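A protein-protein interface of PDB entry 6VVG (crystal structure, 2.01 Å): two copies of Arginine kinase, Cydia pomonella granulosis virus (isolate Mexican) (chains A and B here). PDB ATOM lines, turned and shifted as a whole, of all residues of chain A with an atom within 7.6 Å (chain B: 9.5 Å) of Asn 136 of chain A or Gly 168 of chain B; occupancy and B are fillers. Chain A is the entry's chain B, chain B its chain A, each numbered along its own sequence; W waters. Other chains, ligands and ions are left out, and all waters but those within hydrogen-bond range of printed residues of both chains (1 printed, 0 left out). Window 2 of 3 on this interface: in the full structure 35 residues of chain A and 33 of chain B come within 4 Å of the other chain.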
ATOM      1  N   LEU A  59      -6.497   0.837 -15.553  1.00  0.00           N
ATOM      2  CA  LEU A  59      -5.410   1.774 -15.302  1.00  0.00           C
ATOM      3  C   LEU A  59      -5.371   2.248 -13.855  1.00  0.00           C
ATOM      4  O   LEU A  59      -4.328   2.737 -13.408  1.00  0.00           O
ATOM      5  CB  LEU A  59      -5.527   2.974 -16.241  1.00  0.00           C
ATOM      6  CG  LEU A  59      -4.218   3.691 -16.577  1.00  0.00           C
ATOM      7  CD1 LEU A  59      -3.307   2.794 -17.408  1.00  0.00           C
ATOM      8  CD2 LEU A  59      -4.491   5.008 -17.298  1.00  0.00           C
ATOM      9  N   LEU A  66       2.737   2.176 -10.632  1.00  0.00           N
ATOM     10  CA  LEU A  66       3.735   3.071 -11.208  1.00  0.00           C
ATOM     11  C   LEU A  66       4.182   4.134 -10.214  1.00  0.00           C
ATOM     12  O   LEU A  66       5.344   4.554 -10.240  1.00  0.00           O
ATOM     13  CB  LEU A  66       3.177   3.727 -12.468  1.00  0.00           C
ATOM     14  CG  LEU A  66       2.923   2.787 -13.648  1.00  0.00           C
ATOM     15  CD1 LEU A  66       2.071   3.462 -14.714  1.00  0.00           C
ATOM     16  CD2 LEU A  66       4.253   2.314 -14.227  1.00  0.00           C
ATOM     17  N   ASN A 130       3.176  15.716 -12.239  1.00  0.00           N
ATOM     18  CA  ASN A 130       4.173  15.629 -13.301  1.00  0.00           C
ATOM     19  C   ASN A 130       4.829  14.256 -13.315  1.00  0.00           C
ATOM     20  O   ASN A 130       5.048  13.671 -14.386  1.00  0.00           O
ATOM     21  CB  ASN A 130       5.232  16.720 -13.146  1.00  0.00           C
ATOM     22  CG  ASN A 130       6.207  16.752 -14.315  1.00  0.00           C
ATOM     23  OD1 ASN A 130       5.811  16.949 -15.465  1.00  0.00           O
ATOM     24  ND2 ASN A 130       7.485  16.545 -14.026  1.00  0.00           N
ATOM     25  N   ASP A 131       5.155  13.716 -12.136  1.00  0.00           N
ATOM     26  CA  ASP A 131       5.716  12.376 -12.067  1.00  0.00           C
ATOM     27  C   ASP A 131       4.763  11.351 -12.699  1.00  0.00           C
ATOM     28  O   ASP A 131       5.206  10.457 -13.417  1.00  0.00           O
ATOM     29  CB  ASP A 131       6.025  12.008 -10.617  1.00  0.00           C
ATOM     30  CG  ASP A 131       7.224  12.765 -10.069  1.00  0.00           C
ATOM     31  OD1 ASP A 131       8.034  13.270 -10.877  1.00  0.00           O
ATOM     32  OD2 ASP A 131       7.354  12.861  -8.831  1.00  0.00           O
ATOM     33  N   LEU A 132       3.466  11.496 -12.438  1.00  0.00           N
ATOM     34  CA  LEU A 132       2.501  10.601 -13.078  1.00  0.00           C
ATOM     35  C   LEU A 132       2.513  10.782 -14.588  1.00  0.00           C
ATOM     36  O   LEU A 132       2.462   9.800 -15.339  1.00  0.00           O
ATOM     37  CB  LEU A 132       1.102  10.861 -12.522  1.00  0.00           C
ATOM     38  CG  LEU A 132      -0.033  10.056 -13.153  1.00  0.00           C
ATOM     39  CD1 LEU A 132       0.217   8.563 -12.974  1.00  0.00           C
ATOM     40  CD2 LEU A 132      -1.377  10.453 -12.560  1.00  0.00           C
ATOM     41  N   HIS A 133       2.598  12.030 -15.053  1.00  0.00           N
ATOM     42  CA  HIS A 133       2.556  12.313 -16.482  1.00  0.00           C
ATOM     43  C   HIS A 133       3.770  11.772 -17.227  1.00  0.00           C
ATOM     44  O   HIS A 133       3.711  11.628 -18.452  1.00  0.00           O
ATOM     45  CB  HIS A 133       2.438  13.824 -16.703  1.00  0.00           C
ATOM     46  CG  HIS A 133       1.194  14.422 -16.120  1.00  0.00           C
ATOM     47  ND1 HIS A 133       1.058  15.771 -15.870  1.00  0.00           N
ATOM     48  CD2 HIS A 133       0.027  13.850 -15.739  1.00  0.00           C
ATOM     49  CE1 HIS A 133      -0.140  16.005 -15.365  1.00  0.00           C
ATOM     50  NE2 HIS A 133      -0.786  14.856 -15.275  1.00  0.00           N
ATOM     51  N   LYS A 134       4.867  11.475 -16.528  1.00  0.00           N
ATOM     52  CA  LYS A 134       6.001  10.836 -17.185  1.00  0.00           C
ATOM     53  C   LYS A 134       5.624   9.488 -17.783  1.00  0.00           C
ATOM     54  O   LYS A 134       6.263   9.054 -18.746  1.00  0.00           O
ATOM     55  CB  LYS A 134       7.155  10.673 -16.195  1.00  0.00           C
ATOM     56  CG  LYS A 134       7.793  12.003 -15.792  1.00  0.00           C
ATOM     57  CD  LYS A 134       8.957  11.824 -14.823  1.00  0.00           C
ATOM     58  CE  LYS A 134       9.474  13.180 -14.342  1.00  0.00           C
ATOM     59  NZ  LYS A 134      10.689  13.063 -13.488  1.00  0.00           N
ATOM     60  N   ASN A 135       4.591   8.834 -17.252  1.00  0.00           N
ATOM     61  CA  ASN A 135       4.073   7.586 -17.790  1.00  0.00           C
ATOM     62  C   ASN A 135       3.003   7.809 -18.854  1.00  0.00           C
ATOM     63  O   ASN A 135       2.368   6.844 -19.291  1.00  0.00           O
ATOM     64  CB  ASN A 135       3.501   6.733 -16.654  1.00  0.00           C
ATOM     65  CG  ASN A 135       4.494   6.524 -15.527  1.00  0.00           C
ATOM     66  OD1 ASN A 135       5.349   5.643 -15.597  1.00  0.00           O
ATOM     67  ND2 ASN A 135       4.384   7.332 -14.479  1.00  0.00           N
ATOM     68  N   ASN A 136       2.797   9.058 -19.277  1.00  0.00           N
ATOM     69  CA  ASN A 136       1.734   9.410 -20.218  1.00  0.00           C
ATOM     70  C   ASN A 136       0.371   8.957 -19.701  1.00  0.00           C
ATOM     71  O   ASN A 136      -0.487   8.490 -20.453  1.00  0.00           O
ATOM     72  CB  ASN A 136       2.019   8.844 -21.609  1.00  0.00           C
ATOM     73  CG  ASN A 136       2.700   9.856 -22.518  1.00  0.00           C
ATOM     74  OD1 ASN A 136       2.980  10.984 -22.111  1.00  0.00           O
ATOM     75  ND2 ASN A 136       2.974   9.454 -23.752  1.00  0.00           N
ATOM     76  N   ILE A 137       0.167   9.113 -18.398  1.00  0.00           N
ATOM     77  CA  ILE A 137      -1.123   8.889 -17.761  1.00  0.00           C
ATOM     78  C   ILE A 137      -1.584  10.202 -17.153  1.00  0.00           C
ATOM     79  O   ILE A 137      -0.783  10.949 -16.578  1.00  0.00           O
ATOM     80  CB  ILE A 137      -1.048   7.785 -16.686  1.00  0.00           C
ATOM     81  CG1 ILE A 137      -0.647   6.455 -17.324  1.00  0.00           C
ATOM     82  CG2 ILE A 137      -2.379   7.661 -15.973  1.00  0.00           C
ATOM     83  CD1 ILE A 137      -0.381   5.347 -16.324  1.00  0.00           C
ATOM     84  N   VAL A 138      -2.872  10.494 -17.281  1.00  0.00           N
ATOM     85  CA  VAL A 138      -3.485  11.685 -16.719  1.00  0.00           C
ATOM     86  C   VAL A 138      -4.474  11.245 -15.646  1.00  0.00           C
ATOM     87  O   VAL A 138      -5.276  10.332 -15.884  1.00  0.00           O
ATOM     88  CB  VAL A 138      -4.186  12.504 -17.818  1.00  0.00           C
ATOM     89  CG1 VAL A 138      -5.142  13.522 -17.233  1.00  0.00           C
ATOM     90  CG2 VAL A 138      -3.147  13.164 -18.734  1.00  0.00           C
ATOM     91  N   ARG A 165      -6.538   7.993 -17.458  1.00  0.00           N
ATOM     92  CA  ARG A 165      -6.531   7.698 -18.882  1.00  0.00           C
ATOM     93  C   ARG A 165      -5.129   7.889 -19.445  1.00  0.00           C
ATOM     94  O   ARG A 165      -4.290   8.584 -18.865  1.00  0.00           O
ATOM     95  CB  ARG A 165      -7.518   8.593 -19.648  1.00  0.00           C
ATOM     96  CG  ARG A 165      -8.893   8.700 -19.020  1.00  0.00           C
ATOM     97  CD  ARG A 165      -9.722   7.446 -19.249  1.00  0.00           C
ATOM     98  NE  ARG A 165     -10.991   7.527 -18.532  1.00  0.00           N
ATOM     99  CZ  ARG A 165     -11.756   6.484 -18.232  1.00  0.00           C
ATOM    100  NH1 ARG A 165     -11.390   5.264 -18.593  1.00  0.00           N
ATOM    101  NH2 ARG A 165     -12.891   6.666 -17.568  1.00  0.00           N
ATOM    102  N   ILE A 166      -4.891   7.264 -20.599  1.00  0.00           N
ATOM    103  CA  ILE A 166      -3.621   7.378 -21.304  1.00  0.00           C
ATOM    104  C   ILE A 166      -3.691   8.573 -22.242  1.00  0.00           C
ATOM    105  O   ILE A 166      -4.704   8.799 -22.916  1.00  0.00           O
ATOM    106  CB  ILE A 166      -3.298   6.081 -22.072  1.00  0.00           C
ATOM    107  CG1 ILE A 166      -3.128   4.922 -21.086  1.00  0.00           C
ATOM    108  CG2 ILE A 166      -2.044   6.259 -22.912  1.00  0.00           C
ATOM    109  CD1 ILE A 166      -2.783   3.594 -21.728  1.00  0.00           C
ATOM    110  N   VAL A 167      -2.598   9.338 -22.295  1.00  0.00           N
ATOM    111  CA  VAL A 167      -2.548  10.505 -23.163  1.00  0.00           C
ATOM    112  C   VAL A 167      -2.784  10.088 -24.607  1.00  0.00           C
ATOM    113  O   VAL A 167      -2.268   9.065 -25.076  1.00  0.00           O
ATOM    114  CB  VAL A 167      -1.199  11.224 -23.003  1.00  0.00           C
ATOM    115  CG1 VAL A 167      -1.070  12.349 -24.020  1.00  0.00           C
ATOM    116  CG2 VAL A 167      -1.043  11.748 -21.581  1.00  0.00           C
ATOM    117  N   GLY A 168      -3.587  10.876 -25.315  1.00  0.00           N
ATOM    118  CA  GLY A 168      -3.820  10.658 -26.724  1.00  0.00           C
ATOM    119  C   GLY A 168      -5.030   9.817 -27.064  1.00  0.00           C
ATOM    120  O   GLY A 168      -5.362   9.699 -28.249  1.00  0.00           O
ATOM    121  N   THR A 169      -5.684   9.213 -26.078  1.00  0.00           N
ATOM    122  CA  THR A 169      -6.903   8.470 -26.342  1.00  0.00           C
ATOM    123  C   THR A 169      -8.098   9.421 -26.394  1.00  0.00           C
ATOM    124  O   THR A 169      -8.103  10.459 -25.726  1.00  0.00           O
ATOM    125  CB  THR A 169      -7.136   7.416 -25.264  1.00  0.00           C
ATOM    126  OG1 THR A 169      -7.120   8.031 -23.968  1.00  0.00           O
ATOM    127  CG2 THR A 169      -6.054   6.345 -25.325  1.00  0.00           C
ATOM    128  N   TYR A 190      -7.412  13.087 -24.390  1.00  0.00           N
ATOM    129  CA  TYR A 190      -6.858  13.228 -23.050  1.00  0.00           C
ATOM    130  C   TYR A 190      -5.418  13.719 -23.124  1.00  0.00           C
ATOM    131  O   TYR A 190      -4.639  13.282 -23.975  1.00  0.00           O
ATOM    132  CB  TYR A 190      -6.927  11.897 -22.308  1.00  0.00           C
ATOM    133  CG  TYR A 190      -8.324  11.521 -21.868  1.00  0.00           C
ATOM    134  CD1 TYR A 190      -9.038  12.329 -20.994  1.00  0.00           C
ATOM    135  CD2 TYR A 190      -8.926  10.356 -22.326  1.00  0.00           C
ATOM    136  CE1 TYR A 190     -10.315  11.989 -20.587  1.00  0.00           C
ATOM    137  CE2 TYR A 190     -10.200  10.005 -21.924  1.00  0.00           C
ATOM    138  CZ  TYR A 190     -10.895  10.828 -21.060  1.00  0.00           C
ATOM    139  OH  TYR A 190     -12.167  10.480 -20.662  1.00  0.00           O
ATOM    140  N   THR A 192      -2.193  16.121 -20.643  1.00  0.00           N
ATOM    141  CA  THR A 192      -1.783  16.602 -19.328  1.00  0.00           C
ATOM    142  C   THR A 192      -2.517  17.880 -18.940  1.00  0.00           C
ATOM    143  O   THR A 192      -2.812  18.097 -17.760  1.00  0.00           O
ATOM    144  CB  THR A 192      -0.271  16.845 -19.290  1.00  0.00           C
ATOM    145  OG1 THR A 192       0.093  17.786 -20.309  1.00  0.00           O
ATOM    146  CG2 THR A 192       0.494  15.546 -19.499  1.00  0.00           C
ATOM    147  N   LEU B  59       1.120  -3.028 -16.656  1.00  0.00           N
ATOM    148  CA  LEU B  59       0.411  -2.959 -17.928  1.00  0.00           C
ATOM    149  C   LEU B  59       0.035  -4.337 -18.458  1.00  0.00           C
ATOM    150  O   LEU B  59      -0.872  -4.441 -19.292  1.00  0.00           O
ATOM    151  CB  LEU B  59       1.263  -2.228 -18.964  1.00  0.00           C
ATOM    152  CG  LEU B  59       0.513  -1.479 -20.066  1.00  0.00           C
ATOM    153  CD1 LEU B  59      -0.252  -0.308 -19.476  1.00  0.00           C
ATOM    154  CD2 LEU B  59       1.471  -1.012 -21.154  1.00  0.00           C
ATOM    155  N   ASN B 135      -5.598   1.499 -27.952  1.00  0.00           N
ATOM    156  CA  ASN B 135      -5.509   1.899 -26.553  1.00  0.00           C
ATOM    157  C   ASN B 135      -4.238   2.680 -26.244  1.00  0.00           C
ATOM    158  O   ASN B 135      -4.007   3.020 -25.079  1.00  0.00           O
ATOM    159  CB  ASN B 135      -5.575   0.659 -25.653  1.00  0.00           C
ATOM    160  CG  ASN B 135      -6.818  -0.179 -25.904  1.00  0.00           C
ATOM    161  OD1 ASN B 135      -7.924   0.200 -25.522  1.00  0.00           O
ATOM    162  ND2 ASN B 135      -6.639  -1.326 -26.552  1.00  0.00           N
ATOM    163  N   ASN B 136      -3.423   2.977 -27.259  1.00  0.00           N
ATOM    164  CA  ASN B 136      -2.121   3.622 -27.075  1.00  0.00           C
ATOM    165  C   ASN B 136      -1.211   2.769 -26.193  1.00  0.00           C
ATOM    166  O   ASN B 136      -0.482   3.272 -25.335  1.00  0.00           O
ATOM    167  CB  ASN B 136      -2.278   5.039 -26.518  1.00  0.00           C
ATOM    168  CG  ASN B 136      -2.530   6.064 -27.617  1.00  0.00           C
ATOM    169  OD1 ASN B 136      -2.633   5.712 -28.793  1.00  0.00           O
ATOM    170  ND2 ASN B 136      -2.630   7.334 -27.240  1.00  0.00           N
ATOM    171  N   ILE B 137      -1.255   1.462 -26.422  1.00  0.00           N
ATOM    172  CA  ILE B 137      -0.365   0.499 -25.789  1.00  0.00           C
ATOM    173  C   ILE B 137       0.301  -0.307 -26.895  1.00  0.00           C
ATOM    174  O   ILE B 137      -0.343  -0.656 -27.890  1.00  0.00           O
ATOM    175  CB  ILE B 137      -1.132  -0.429 -24.824  1.00  0.00           C
ATOM    176  CG1 ILE B 137      -1.760   0.387 -23.692  1.00  0.00           C
ATOM    177  CG2 ILE B 137      -0.212  -1.499 -24.269  1.00  0.00           C
ATOM    178  CD1 ILE B 137      -2.645  -0.420 -22.758  1.00  0.00           C
ATOM    179  N   VAL B 138       1.588  -0.603 -26.726  1.00  0.00           N
ATOM    180  CA  VAL B 138       2.317  -1.462 -27.652  1.00  0.00           C
ATOM    181  C   VAL B 138       2.683  -2.750 -26.928  1.00  0.00           C
ATOM    182  O   VAL B 138       2.924  -2.760 -25.715  1.00  0.00           O
ATOM    183  CB  VAL B 138       3.578  -0.779 -28.223  1.00  0.00           C
ATOM    184  CG1 VAL B 138       3.180   0.312 -29.211  1.00  0.00           C
ATOM    185  CG2 VAL B 138       4.438  -0.222 -27.104  1.00  0.00           C
ATOM    186  N   ARG B 165       3.993  -1.611 -23.138  1.00  0.00           N
ATOM    187  CA  ARG B 165       4.309  -0.249 -22.740  1.00  0.00           C
ATOM    188  C   ARG B 165       3.283   0.738 -23.280  1.00  0.00           C
ATOM    189  O   ARG B 165       2.591   0.482 -24.270  1.00  0.00           O
ATOM    190  CB  ARG B 165       5.700   0.181 -23.239  1.00  0.00           C
ATOM    191  CG  ARG B 165       6.838  -0.744 -22.874  1.00  0.00           C
ATOM    192  CD  ARG B 165       7.177  -0.641 -21.396  1.00  0.00           C
ATOM    193  NE  ARG B 165       8.165  -1.648 -21.028  1.00  0.00           N
ATOM    194  CZ  ARG B 165       8.264  -2.205 -19.826  1.00  0.00           C
ATOM    195  NH1 ARG B 165       7.443  -1.840 -18.852  1.00  0.00           N
ATOM    196  NH2 ARG B 165       9.196  -3.123 -19.600  1.00  0.00           N
ATOM    197  N   ILE B 166       3.221   1.895 -22.622  1.00  0.00           N
ATOM    198  CA  ILE B 166       2.353   2.987 -23.047  1.00  0.00           C
ATOM    199  C   ILE B 166       3.052   3.787 -24.138  1.00  0.00           C
ATOM    200  O   ILE B 166       4.233   4.134 -24.013  1.00  0.00           O
ATOM    201  CB  ILE B 166       1.987   3.892 -21.859  1.00  0.00           C
ATOM    202  CG1 ILE B 166       1.106   3.150 -20.854  1.00  0.00           C
ATOM    203  CG2 ILE B 166       1.284   5.147 -22.350  1.00  0.00           C
ATOM    204  CD1 ILE B 166       0.785   3.953 -19.597  1.00  0.00           C
ATOM    205  N   VAL B 167       2.315   4.093 -25.209  1.00  0.00           N
ATOM    206  CA  VAL B 167       2.878   4.863 -26.311  1.00  0.00           C
ATOM    207  C   VAL B 167       3.362   6.210 -25.801  1.00  0.00           C
ATOM    208  O   VAL B 167       2.654   6.906 -25.062  1.00  0.00           O
ATOM    209  CB  VAL B 167       1.832   5.034 -27.424  1.00  0.00           C
ATOM    210  CG1 VAL B 167       2.316   6.028 -28.472  1.00  0.00           C
ATOM    211  CG2 VAL B 167       1.500   3.691 -28.056  1.00  0.00           C
ATOM    212  N   GLY B 168       4.580   6.582 -26.190  1.00  0.00           N
ATOM    213  CA  GLY B 168       5.117   7.895 -25.898  1.00  0.00           C
ATOM    214  C   GLY B 168       6.070   7.967 -24.723  1.00  0.00           C
ATOM    215  O   GLY B 168       6.721   9.005 -24.545  1.00  0.00           O
ATOM    216  N   THR B 169       6.180   6.911 -23.927  1.00  0.00           N
ATOM    217  CA  THR B 169       7.056   6.924 -22.768  1.00  0.00           C
ATOM    218  C   THR B 169       8.490   6.601 -23.172  1.00  0.00           C
ATOM    219  O   THR B 169       8.730   5.993 -24.219  1.00  0.00           O
ATOM    220  CB  THR B 169       6.569   5.919 -21.732  1.00  0.00           C
ATOM    221  OG1 THR B 169       6.499   4.611 -22.315  1.00  0.00           O
ATOM    222  CG2 THR B 169       5.192   6.320 -21.216  1.00  0.00           C
ATOM    223  N   PRO B 170       9.468   7.012 -22.363  1.00  0.00           N
ATOM    224  CA  PRO B 170      10.871   6.732 -22.709  1.00  0.00           C
ATOM    225  C   PRO B 170      11.134   5.234 -22.764  1.00  0.00           C
ATOM    226  O   PRO B 170      10.711   4.478 -21.888  1.00  0.00           O
ATOM    227  CB  PRO B 170      11.665   7.405 -21.579  1.00  0.00           C
ATOM    228  CG  PRO B 170      10.719   8.441 -20.992  1.00  0.00           C
ATOM    229  CD  PRO B 170       9.339   7.819 -21.133  1.00  0.00           C
ATOM    230  N   SER B 171      11.860   4.810 -23.789  1.00  0.00           N
ATOM    231  CA  SER B 171      12.136   3.394 -23.967  1.00  0.00           C
ATOM    232  C   SER B 171      13.482   3.020 -23.351  1.00  0.00           C
ATOM    233  O   SER B 171      14.359   3.861 -23.142  1.00  0.00           O
ATOM    234  CB  SER B 171      12.125   3.022 -25.449  1.00  0.00           C
ATOM    235  OG  SER B 171      13.232   3.596 -26.121  1.00  0.00           O
ATOM    236  N   HIS B 187      16.750   4.481 -28.819  1.00  0.00           N
ATOM    237  CA  HIS B 187      16.055   4.963 -27.626  1.00  0.00           C
ATOM    238  C   HIS B 187      14.991   6.010 -27.962  1.00  0.00           C
ATOM    239  O   HIS B 187      14.812   6.988 -27.235  1.00  0.00           O
ATOM    240  CB  HIS B 187      17.041   5.528 -26.597  1.00  0.00           C
ATOM    241  CG  HIS B 187      17.922   4.494 -25.964  1.00  0.00           C
ATOM    242  ND1 HIS B 187      17.463   3.597 -25.022  1.00  0.00           N
ATOM    243  CD2 HIS B 187      19.236   4.220 -26.133  1.00  0.00           C
ATOM    244  CE1 HIS B 187      18.456   2.812 -24.644  1.00  0.00           C
ATOM    245  NE2 HIS B 187      19.542   3.170 -25.303  1.00  0.00           N
ATOM    246  N   GLU B 188      14.278   5.808 -29.066  1.00  0.00           N
ATOM    247  CA  GLU B 188      13.077   6.593 -29.306  1.00  0.00           C
ATOM    248  C   GLU B 188      11.966   6.139 -28.362  1.00  0.00           C
ATOM    249  O   GLU B 188      12.003   5.039 -27.803  1.00  0.00           O
ATOM    250  CB  GLU B 188      12.624   6.461 -30.760  1.00  0.00           C
ATOM    251  CG  GLU B 188      13.568   7.086 -31.770  1.00  0.00           C
ATOM    252  CD  GLU B 188      12.922   7.284 -33.135  1.00  0.00           C
ATOM    253  OE1 GLU B 188      11.678   7.227 -33.234  1.00  0.00           O
ATOM    254  OE2 GLU B 188      13.664   7.488 -34.113  1.00  0.00           O
ATOM    255  N   ALA B 189      10.968   7.002 -28.186  1.00  0.00           N
ATOM    256  CA  ALA B 189       9.834   6.661 -27.336  1.00  0.00           C
ATOM    257  C   ALA B 189       9.124   5.417 -27.864  1.00  0.00           C
ATOM    258  O   ALA B 189       9.132   5.132 -29.064  1.00  0.00           O
ATOM    259  CB  ALA B 189       8.852   7.830 -27.264  1.00  0.00           C
ATOM    260  N   TYR B 190       8.515   4.662 -26.948  1.00  0.00           N
ATOM    261  CA  TYR B 190       7.715   3.511 -27.345  1.00  0.00           C
ATOM    262  C   TYR B 190       6.638   3.944 -28.332  1.00  0.00           C
ATOM    263  O   TYR B 190       5.923   4.922 -28.102  1.00  0.00           O
ATOM    264  CB  TYR B 190       7.086   2.855 -26.114  1.00  0.00           C
ATOM    265  CG  TYR B 190       8.078   2.053 -25.305  1.00  0.00           C
ATOM    266  CD1 TYR B 190       8.796   1.010 -25.884  1.00  0.00           C
ATOM    267  CD2 TYR B 190       8.303   2.338 -23.967  1.00  0.00           C
ATOM    268  CE1 TYR B 190       9.712   0.279 -25.152  1.00  0.00           C
ATOM    269  CE2 TYR B 190       9.215   1.608 -23.225  1.00  0.00           C
ATOM    270  CZ  TYR B 190       9.922   0.584 -23.824  1.00  0.00           C
ATOM    271  OH  TYR B 190      10.830  -0.145 -23.091  1.00  0.00           O
ATOM    272  N   GLN B 191       6.535   3.218 -29.443  1.00  0.00           N
ATOM    273  CA  GLN B 191       5.630   3.594 -30.518  1.00  0.00           C
ATOM    274  C   GLN B 191       5.202   2.339 -31.262  1.00  0.00           C
ATOM    275  O   GLN B 191       5.833   1.285 -31.151  1.00  0.00           O
ATOM    276  CB  GLN B 191       6.289   4.592 -31.476  1.00  0.00           C
ATOM    277  CG  GLN B 191       7.734   4.257 -31.815  1.00  0.00           C
ATOM    278  CD  GLN B 191       8.402   5.326 -32.662  1.00  0.00           C
ATOM    279  OE1 GLN B 191       8.220   5.373 -33.880  1.00  0.00           O
ATOM    280  NE2 GLN B 191       9.185   6.186 -32.022  1.00  0.00           N
ATOM    281  N   THR B 192       4.110   2.464 -32.019  1.00  0.00           N
ATOM    282  CA  THR B 192       3.581   1.306 -32.733  1.00  0.00           C
ATOM    283  C   THR B 192       4.607   0.731 -33.701  1.00  0.00           C
ATOM    284  O   THR B 192       4.615  -0.480 -33.946  1.00  0.00           O
ATOM    285  CB  THR B 192       2.302   1.678 -33.487  1.00  0.00           C
ATOM    286  OG1 THR B 192       2.556   2.775 -34.374  1.00  0.00           O
ATOM    287  CG2 THR B 192       1.194   2.060 -32.512  1.00  0.00           C
ATOM    288  N   PHE B 194       7.596   0.100 -33.295  1.00  0.00           N
ATOM    289  CA  PHE B 194       8.345  -0.958 -32.621  1.00  0.00           C
ATOM    290  C   PHE B 194       7.723  -2.316 -32.916  1.00  0.00           C
ATOM    291  O   PHE B 194       8.412  -3.268 -33.306  1.00  0.00           O
ATOM    292  CB  PHE B 194       8.362  -0.729 -31.107  1.00  0.00           C
ATOM    293  CG  PHE B 194       9.283   0.361 -30.647  1.00  0.00           C
ATOM    294  CD1 PHE B 194       9.660   1.386 -31.492  1.00  0.00           C
ATOM    295  CD2 PHE B 194       9.761   0.360 -29.344  1.00  0.00           C
ATOM    296  CE1 PHE B 194      10.502   2.386 -31.052  1.00  0.00           C
ATOM    297  CE2 PHE B 194      10.602   1.357 -28.899  1.00  0.00           C
ATOM    298  CZ  PHE B 194      10.973   2.371 -29.752  1.00  0.00           C
HETATM  299  O   HOH W   1       0.065   7.912 -25.484  1.00  0.00           O
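The backbone carbonyl oxygen (O) of Val 167 of chain A sits at hydrogen-bond distance from the side-chain amide nitrogen (ND2) of Asn 136 of chain B, 2.8 Å away.
The side-chain amide nitrogen (ND2) of Asn 136 of chain A lies within hydrogen-bond range of the backbone carbonyl oxygen (O) of Val 167 of chain B (2.9 Å).
O of Ile 166 of chain B sits at hydrogen-bond distance from OG1 of Thr 169 of chain B (2.9 Å).
The backbone carbonyl oxygen of Tyr 190 of chain B sits at hydrogen-bond distance from the backbone NH of Gly 168 of chain B (2.9 Å).
The side-chain amide nitrogen (ND2) of Asn 135 of chain A lies within hydrogen-bond range of the backbone carbonyl oxygen (O) of Asp 131 of chain A.
O of Leu 132 of chain A is in hydrogen-bond range of ND2 of Asn 135 of chain A, 3.2 Å away.
N of Val 167 of chain A is in hydrogen-bond range of O of Asn 136 of chain A.
The backbone carbonyl oxygen (O) of Thr 169 of chain A sits at hydrogen-bond distance from the backbone NH (N) of Tyr 190 of chain A, at 3.0 Å.
Lys 134 of chain A touches Thr 169 of chain B.
CG2 of Thr 169 of chain B touches O of Asn 135 of chain A, at 3.5 Å.
Ile 166 of chain B touches Asn 136 of chain A (CG2 to CB, 3.8 Å).
Ile 166 of chain B touches Ile 137 of chain A.
Asn 135 of chain B touches Ile 166 of chain A (O to CD1, 3.6 Å).
Asn 136 of chain B touches Ile 166 of chain A (CB to CG2, 3.8 Å).
Ile 166 of chain A touches Ile 137 of chain B (CD1 to CG1, 3.9 Å).
CG2 of Ile 166 of chain A touches CG2 of Ile 166 of chain B, 3.6 Å away.
Asn 136 of chain B touches Gly 168 of chain A (ND2 to C, 3.5 Å).
Asn 136 of chain B touches Thr 169 of chain A.
Printed residues of chain B within 4 Å of Lys 134 of chain A: Thr 169 (3.8 Å).
Asn 136 of chain A touches three residues of chain B.
Ile 137 of chain A touches just one residue of chain B: Ile 166 (3.7 Å).
Of chain B, only Asn 136 comes within 4 Å of Val 167 of chain A.
Printed residues of chain A within 4 Å of Ile 137 of chain B: Ile 166.
Printed residues of chain A within 4 Å of Ile 166 of chain B: Asn 135 (3.3 Å), Asn 136 (3.8 Å), Ile 137 (3.7 Å) and Ile 166 (3.6 Å).
Of the printed residues of chain A, Val 167 of chain B touches Asn 136 (2.9 Å).
Gly 168 of chain B touches just one residue of chain A: Asn 136.
The nearest residue of chain A that does not touch Gly 168 of chain B is Lys 134 of chain A (5.8 Å).
The nearest printed residue of chain A that does not touch Ile 137 of chain B is Leu 59 of chain A (6.3 Å).
Of the 18 printed residues of chain A, 8 touch a printed residue of chain B.
Hydrophobic or aromatic side chains of chain A within 4 Å of the printed part of chain B: Ile 137 and Ile 166.
Along chain A the printed residues that touch a printed residue of chain B span positions 134 to 169.
Hydrophobic or aromatic side chains of chain B within 4 Å of the printed part of chain A: Ile 137 and Ile 166.
Along chain B the printed residues that touch a printed residue of chain A span positions 135 to 169.
Asn 135 of chain A touches Thr 169 of chain B, and with the chains exchanged Thr 169 of chain A touches Asn 135 of chain B.
Ile 137 of chain A touches Ile 166 of chain B, and with the chains exchanged Ile 166 of chain A touches Ile 137 of chain B.
Ile 166 of chain A touches its own counterpart, Ile 166 of chain B.
Thr 169 of chain A touches Asn 136 of chain B, but with the chains exchanged Asn 136 of chain A does not touch Thr 169 of chain B (4.1 Å).
Positions printed for both chains: 59, 135, 136, 137, 138, 165, 166, 167, 168, 169, 190 and 192.
Water W1 lies within hydrogen-bond range of O of Val 167 of chain A (2.6 Å), O of Val 167 of chain B (2.8 Å) and ND2 of Asn 136 of chain B (3.3 Å).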
